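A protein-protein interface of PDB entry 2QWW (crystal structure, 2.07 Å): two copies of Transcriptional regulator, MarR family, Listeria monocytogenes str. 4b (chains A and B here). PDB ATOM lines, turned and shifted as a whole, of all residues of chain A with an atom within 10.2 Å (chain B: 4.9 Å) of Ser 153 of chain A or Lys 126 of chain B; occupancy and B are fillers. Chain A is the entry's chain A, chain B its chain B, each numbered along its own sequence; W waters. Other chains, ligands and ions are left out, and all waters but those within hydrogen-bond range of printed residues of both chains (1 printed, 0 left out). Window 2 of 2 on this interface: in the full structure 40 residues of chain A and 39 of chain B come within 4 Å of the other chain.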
ATOM      1  N   ASP A   8      18.477  31.694  -3.118  1.00  0.00           N
ATOM      2  CA  ASP A   8      17.515  30.792  -3.783  1.00  0.00           C
ATOM      3  C   ASP A   8      17.158  31.238  -5.181  1.00  0.00           C
ATOM      4  O   ASP A   8      17.012  30.415  -6.072  1.00  0.00           O
ATOM      5  CB  ASP A   8      16.251  30.559  -2.947  1.00  0.00           C
ATOM      6  CG  ASP A   8      16.440  29.456  -1.907  1.00  0.00           C
ATOM      7  OD1 ASP A   8      17.593  29.222  -1.478  1.00  0.00           O
ATOM      8  OD2 ASP A   8      15.436  28.818  -1.521  1.00  0.00           O
ATOM      9  N   ILE A  12      17.527  28.948  -8.492  1.00  0.00           N
ATOM     10  CA  ILE A  12      16.399  28.691  -9.392  1.00  0.00           C
ATOM     11  C   ILE A  12      16.846  29.019 -10.807  1.00  0.00           C
ATOM     12  O   ILE A  12      16.691  28.210 -11.703  1.00  0.00           O
ATOM     13  CB  ILE A  12      15.120  29.493  -8.981  1.00  0.00           C
ATOM     14  CG1 ILE A  12      14.552  28.943  -7.674  1.00  0.00           C
ATOM     15  CG2 ILE A  12      14.026  29.420 -10.067  1.00  0.00           C
ATOM     16  CD1 ILE A  12      13.462  29.795  -7.047  1.00  0.00           C
ATOM     17  N   LYS A 145      11.686  14.110  -8.134  1.00  0.00           N
ATOM     18  CA  LYS A 145      11.111  14.856  -7.028  1.00  0.00           C
ATOM     19  C   LYS A 145      10.614  16.210  -7.514  1.00  0.00           C
ATOM     20  O   LYS A 145       9.502  16.637  -7.185  1.00  0.00           O
ATOM     21  CB  LYS A 145      12.136  15.008  -5.908  1.00  0.00           C
ATOM     22  CG  LYS A 145      11.621  15.636  -4.639  1.00  0.00           C
ATOM     23  CD  LYS A 145      12.679  15.584  -3.538  1.00  0.00           C
ATOM     24  CE  LYS A 145      12.725  14.241  -2.841  1.00  0.00           C
ATOM     25  NZ  LYS A 145      11.525  14.033  -1.980  1.00  0.00           N
ATOM     26  N   VAL A 146      11.428  16.864  -8.329  1.00  0.00           N
ATOM     27  CA  VAL A 146      11.087  18.175  -8.859  1.00  0.00           C
ATOM     28  C   VAL A 146       9.791  18.123  -9.690  1.00  0.00           C
ATOM     29  O   VAL A 146       8.920  18.974  -9.538  1.00  0.00           O
ATOM     30  CB  VAL A 146      12.260  18.812  -9.671  1.00  0.00           C
ATOM     31  CG1 VAL A 146      11.835  20.141 -10.306  1.00  0.00           C
ATOM     32  CG2 VAL A 146      13.472  19.061  -8.776  1.00  0.00           C
ATOM     33  N   GLU A 147       9.691  17.139 -10.568  1.00  0.00           N
ATOM     34  CA  GLU A 147       8.523  16.929 -11.400  1.00  0.00           C
ATOM     35  C   GLU A 147       7.289  16.705 -10.538  1.00  0.00           C
ATOM     36  O   GLU A 147       6.246  17.294 -10.793  1.00  0.00           O
ATOM     37  CB  GLU A 147       8.735  15.695 -12.270  1.00  0.00           C
ATOM     38  CG  GLU A 147       7.567  15.340 -13.169  1.00  0.00           C
ATOM     39  CD  GLU A 147       7.647  13.925 -13.721  1.00  0.00           C
ATOM     40  OE1 GLU A 147       8.687  13.250 -13.537  1.00  0.00           O
ATOM     41  OE2 GLU A 147       6.659  13.485 -14.355  1.00  0.00           O
ATOM     42  N   THR A 148       7.421  15.857  -9.515  1.00  0.00           N
ATOM     43  CA  THR A 148       6.301  15.532  -8.636  1.00  0.00           C
ATOM     44  C   THR A 148       5.811  16.760  -7.896  1.00  0.00           C
ATOM     45  O   THR A 148       4.606  16.988  -7.812  1.00  0.00           O
ATOM     46  CB  THR A 148       6.629  14.365  -7.669  1.00  0.00           C
ATOM     47  OG1 THR A 148       7.848  14.629  -6.987  1.00  0.00           O
ATOM     48  CG2 THR A 148       6.823  13.082  -8.427  1.00  0.00           C
ATOM     49  N   LEU A 149       6.731  17.572  -7.400  1.00  0.00           N
ATOM     50  CA  LEU A 149       6.369  18.794  -6.696  1.00  0.00           C
ATOM     51  C   LEU A 149       5.769  19.859  -7.610  1.00  0.00           C
ATOM     52  O   LEU A 149       4.943  20.651  -7.167  1.00  0.00           O
ATOM     53  CB  LEU A 149       7.584  19.363  -5.965  1.00  0.00           C
ATOM     54  CG  LEU A 149       8.093  18.505  -4.812  1.00  0.00           C
ATOM     55  CD1 LEU A 149       9.420  19.055  -4.287  1.00  0.00           C
ATOM     56  CD2 LEU A 149       7.024  18.420  -3.691  1.00  0.00           C
ATOM     57  N   LEU A 150       6.227  19.921  -8.857  1.00  0.00           N
ATOM     58  CA  LEU A 150       5.665  20.851  -9.849  1.00  0.00           C
ATOM     59  C   LEU A 150       4.202  20.539 -10.133  1.00  0.00           C
ATOM     60  O   LEU A 150       3.378  21.442 -10.221  1.00  0.00           O
ATOM     61  CB  LEU A 150       6.443  20.782 -11.164  1.00  0.00           C
ATOM     62  CG  LEU A 150       7.776  21.520 -11.214  1.00  0.00           C
ATOM     63  CD1 LEU A 150       8.545  21.093 -12.471  1.00  0.00           C
ATOM     64  CD2 LEU A 150       7.564  23.005 -11.166  1.00  0.00           C
ATOM     65  N   LYS A 151       3.898  19.249 -10.252  1.00  0.00           N
ATOM     66  CA  LYS A 151       2.549  18.771 -10.487  1.00  0.00           C
ATOM     67  C   LYS A 151       1.579  18.977  -9.331  1.00  0.00           C
ATOM     68  O   LYS A 151       0.383  18.785  -9.521  1.00  0.00           O
ATOM     69  CB  LYS A 151       2.568  17.270 -10.841  1.00  0.00           C
ATOM     70  CG  LYS A 151       3.152  16.965 -12.174  1.00  0.00           C
ATOM     71  CD  LYS A 151       3.236  15.449 -12.420  1.00  0.00           C
ATOM     72  CE  LYS A 151       3.670  15.169 -13.851  1.00  0.00           C
ATOM     73  NZ  LYS A 151       3.806  13.705 -14.159  1.00  0.00           N
ATOM     74  N   LYS A 152       2.065  19.349  -8.147  1.00  0.00           N
ATOM     75  CA  LYS A 152       1.192  19.560  -6.987  1.00  0.00           C
ATOM     76  C   LYS A 152       0.564  20.948  -6.924  1.00  0.00           C
ATOM     77  O   LYS A 152      -0.647  21.061  -6.725  1.00  0.00           O
ATOM     78  CB  LYS A 152       1.937  19.251  -5.680  1.00  0.00           C
ATOM     79  CG  LYS A 152       2.179  17.764  -5.512  1.00  0.00           C
ATOM     80  CD  LYS A 152       3.018  17.429  -4.293  1.00  0.00           C
ATOM     81  CE  LYS A 152       3.190  15.913  -4.159  1.00  0.00           C
ATOM     82  NZ  LYS A 152       4.065  15.570  -3.004  1.00  0.00           N
ATOM     83  N   SER A 153       1.373  21.996  -7.082  1.00  0.00           N
ATOM     84  CA  SER A 153       0.873  23.379  -7.012  1.00  0.00           C
ATOM     85  C   SER A 153       0.074  23.742  -8.255  1.00  0.00           C
ATOM     86  O   SER A 153       0.575  23.622  -9.370  1.00  0.00           O
ATOM     87  CB  SER A 153       2.029  24.364  -6.846  1.00  0.00           C
ATOM     88  N   TYR B  29       4.011  27.509 -18.067  1.00  0.00           N
ATOM     89  CA  TYR B  29       4.414  28.731 -17.395  1.00  0.00           C
ATOM     90  C   TYR B  29       4.960  29.743 -18.389  1.00  0.00           C
ATOM     91  O   TYR B  29       4.895  30.937 -18.160  1.00  0.00           O
ATOM     92  CB  TYR B  29       5.433  28.438 -16.290  1.00  0.00           C
ATOM     93  CG  TYR B  29       4.832  27.688 -15.141  1.00  0.00           C
ATOM     94  CD1 TYR B  29       3.831  28.264 -14.374  1.00  0.00           C
ATOM     95  CD2 TYR B  29       5.267  26.424 -14.798  1.00  0.00           C
ATOM     96  CE1 TYR B  29       3.262  27.591 -13.324  1.00  0.00           C
ATOM     97  CE2 TYR B  29       4.707  25.745 -13.736  1.00  0.00           C
ATOM     98  CZ  TYR B  29       3.710  26.334 -13.000  1.00  0.00           C
ATOM     99  OH  TYR B  29       3.140  25.676 -11.939  1.00  0.00           O
ATOM    100  N   LYS B 122       7.958  31.608  -9.249  1.00  0.00           N
ATOM    101  CA  LYS B 122       7.068  31.343  -8.122  1.00  0.00           C
ATOM    102  C   LYS B 122       6.860  29.845  -7.976  1.00  0.00           C
ATOM    103  O   LYS B 122       6.865  29.320  -6.875  1.00  0.00           O
ATOM    104  CB  LYS B 122       5.715  32.024  -8.310  1.00  0.00           C
ATOM    105  N   ALA B 123       6.696  29.160  -9.091  1.00  0.00           N
ATOM    106  CA  ALA B 123       6.487  27.715  -9.076  1.00  0.00           C
ATOM    107  C   ALA B 123       7.713  26.947  -8.573  1.00  0.00           C
ATOM    108  O   ALA B 123       7.589  26.041  -7.767  1.00  0.00           O
ATOM    109  CB  ALA B 123       6.121  27.245 -10.458  1.00  0.00           C
ATOM    110  N   MET B 124       8.896  27.302  -9.054  1.00  0.00           N
ATOM    111  CA  MET B 124      10.120  26.626  -8.627  1.00  0.00           C
ATOM    112  C   MET B 124      10.447  26.974  -7.176  1.00  0.00           C
ATOM    113  O   MET B 124      10.994  26.168  -6.450  1.00  0.00           O
ATOM    114  CB  MET B 124      11.285  26.981  -9.555  1.00  0.00           C
ATOM    115  CG  MET B 124      12.386  25.931  -9.587  1.00  0.00           C
ATOM    116  SD  MET B 124      11.733  24.182 -10.191  1.00  0.00           S
ATOM    117  CE  MET B 124      11.036  24.706 -11.668  1.00  0.00           C
ATOM    118  N   MET B 125      10.097  28.185  -6.765  1.00  0.00           N
ATOM    119  CA  MET B 125      10.240  28.617  -5.386  1.00  0.00           C
ATOM    120  C   MET B 125       9.431  27.726  -4.431  1.00  0.00           C
ATOM    121  O   MET B 125       9.900  27.383  -3.358  1.00  0.00           O
ATOM    122  CB  MET B 125       9.789  30.065  -5.288  1.00  0.00           C
ATOM    123  CG  MET B 125       9.698  30.625  -3.906  1.00  0.00           C
ATOM    124  SD  MET B 125       9.362  32.512  -4.030  1.00  0.00           S
ATOM    125  CE  MET B 125      10.829  33.122  -5.342  1.00  0.00           C
ATOM    126  N   LYS B 126       8.222  27.345  -4.823  1.00  0.00           N
ATOM    127  CA  LYS B 126       7.419  26.435  -4.013  1.00  0.00           C
ATOM    128  C   LYS B 126       8.066  25.053  -3.966  1.00  0.00           C
ATOM    129  O   LYS B 126       7.988  24.362  -2.955  1.00  0.00           O
ATOM    130  CB  LYS B 126       6.000  26.296  -4.568  1.00  0.00           C
ATOM    131  CG  LYS B 126       5.178  27.562  -4.546  1.00  0.00           C
ATOM    132  CD  LYS B 126       3.916  27.402  -5.405  1.00  0.00           C
ATOM    133  CE  LYS B 126       3.093  28.682  -5.461  1.00  0.00           C
ATOM    134  NZ  LYS B 126       1.862  28.485  -6.282  1.00  0.00           N
ATOM    135  N   VAL B 127       8.677  24.644  -5.072  1.00  0.00           N
ATOM    136  CA  VAL B 127       9.350  23.336  -5.149  1.00  0.00           C
ATOM    137  C   VAL B 127      10.489  23.268  -4.138  1.00  0.00           C
ATOM    138  O   VAL B 127      10.602  22.300  -3.392  1.00  0.00           O
ATOM    139  CB  VAL B 127       9.871  23.069  -6.574  1.00  0.00           C
ATOM    140  CG1 VAL B 127      10.777  21.817  -6.638  1.00  0.00           C
ATOM    141  CG2 VAL B 127       8.697  22.917  -7.528  1.00  0.00           C
ATOM    142  N   PHE B 128      11.283  24.340  -4.102  1.00  0.00           N
ATOM    143  CA  PHE B 128      12.444  24.499  -3.227  1.00  0.00           C
ATOM    144  C   PHE B 128      12.110  24.463  -1.731  1.00  0.00           C
ATOM    145  O   PHE B 128      12.909  23.968  -0.935  1.00  0.00           O
ATOM    146  CB  PHE B 128      13.211  25.782  -3.618  1.00  0.00           C
ATOM    147  CG  PHE B 128      14.180  25.596  -4.775  1.00  0.00           C
ATOM    148  CD1 PHE B 128      13.909  24.726  -5.829  1.00  0.00           C
ATOM    149  CD2 PHE B 128      15.354  26.316  -4.822  1.00  0.00           C
ATOM    150  CE1 PHE B 128      14.812  24.568  -6.869  1.00  0.00           C
ATOM    151  CE2 PHE B 128      16.237  26.169  -5.867  1.00  0.00           C
ATOM    152  CZ  PHE B 128      15.971  25.286  -6.885  1.00  0.00           C
ATOM    153  N   GLU B 129      10.936  24.963  -1.354  1.00  0.00           N
ATOM    154  CA  GLU B 129      10.460  24.877   0.026  1.00  0.00           C
ATOM    155  C   GLU B 129      10.259  23.411   0.451  1.00  0.00           C
ATOM    156  O   GLU B 129      10.254  23.089   1.641  1.00  0.00           O
ATOM    157  CB  GLU B 129       9.161  25.660   0.185  1.00  0.00           C
ATOM    158  CG  GLU B 129       9.356  27.182   0.180  1.00  0.00           C
ATOM    159  CD  GLU B 129       8.068  27.950  -0.097  1.00  0.00           C
ATOM    160  OE1 GLU B 129       7.008  27.311  -0.322  1.00  0.00           O
ATOM    161  OE2 GLU B 129       8.120  29.205  -0.098  1.00  0.00           O
ATOM    162  N   ASN B 130      10.064  22.541  -0.531  1.00  0.00           N
ATOM    163  CA  ASN B 130       9.935  21.106  -0.307  1.00  0.00           C
ATOM    164  C   ASN B 130      11.164  20.295  -0.691  1.00  0.00           C
ATOM    165  O   ASN B 130      11.097  19.073  -0.834  1.00  0.00           O
ATOM    166  CB  ASN B 130       8.684  20.596  -1.001  1.00  0.00           C
ATOM    167  CG  ASN B 130       7.417  21.016  -0.274  1.00  0.00           C
ATOM    168  OD1 ASN B 130       7.268  20.762   0.926  1.00  0.00           O
ATOM    169  ND2 ASN B 130       6.497  21.642  -0.993  1.00  0.00           N
HETATM  170  O   HOH W   1      12.509  16.155  -0.409  1.00  0.00           O
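Ile 12 of chain A touches Met 124 of chain B (CG2 to CB, 3.7 Å). Met 125 of chain B touches Ile 12 of chain A (N to CD1, 3.7 Å). Phe 128 of chain B touches Ile 12 of chain A (CE2 to CG1, 3.7 Å). Leu 149 of chain A touches Val 127 of chain B (CD1 to O, 3.6 Å). Leu 149 of chain A touches Asn 130 of chain B (CD1 to CB, 3.7 Å). Leu 150 of chain A touches Met 124 of chain B (CD2 to CE, 3.9 Å). Leu 150 of chain A touches Val 127 of chain B. Ser 153 of chain A touches Lys 126 of chain B (CB to CD, 3.9 Å).
Of chain B, only Lys 126 (3.9 Å) comes within 4 Å of Ser 153 of chain A. Of chain A, only Ser 153 (3.9 Å) comes within 4 Å of Lys 126 of chain B. No residue of chain A comes within 4 Å of Glu 129 of chain B. Printed residues of chain A within 4 Å of Met 125 of chain B: Ile 12. Of the printed residues of chain A, Met 124 of chain B touches Ile 12 (3.7 Å) and Leu 150 (3.9 Å). Printed residues of chain A within 4 Å of Asn 130 of chain B: Leu 149 (3.7 Å). Printed residues of chain B within 4 Å of Ile 12 of chain A: Met 124 (3.7 Å), Met 125 (3.7 Å) and Phe 128 (3.7 Å). Of the printed residues of chain B, Leu 149 of chain A touches Val 127 and Asn 130. The nearest residue of chain A that does not touch Lys 126 of chain B is Leu 149 of chain A (5.7 Å).
No position is printed for both chains. Of the 8 pairs that touch across the chains among the printed residues, none has its exchanged pair printed and touching as well.
Water W1 lies within hydrogen-bond range of NZ of Lys 145 of chain A (2.8 Å) and O of Asn 130 of chain B (3.3 Å).
Printed residues of chain A that touch a printed residue of chain B: Ile 12, Leu 149, Leu 150 and Ser 153. Hydrophobic or aromatic side chains of chain A within 4 Å of the printed part of chain B: Ile 12, Leu 149 and Leu 150. Of the 10 printed residues of chain B, 6 touch a printed residue of chain A. Printed residues of chain B that touch a printed residue of chain A: Met 124, Met 125, Lys 126, Val 127, Phe 128 and Asn 130. Hydrophobic or aromatic side chains of chain B that line the printed part of chain A: Met 124, Val 127 and Phe 128. Among the printed residues, no Asp or Glu carboxylate lies within 4 Å of a Lys or Arg side-chain nitrogen of the other chain.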
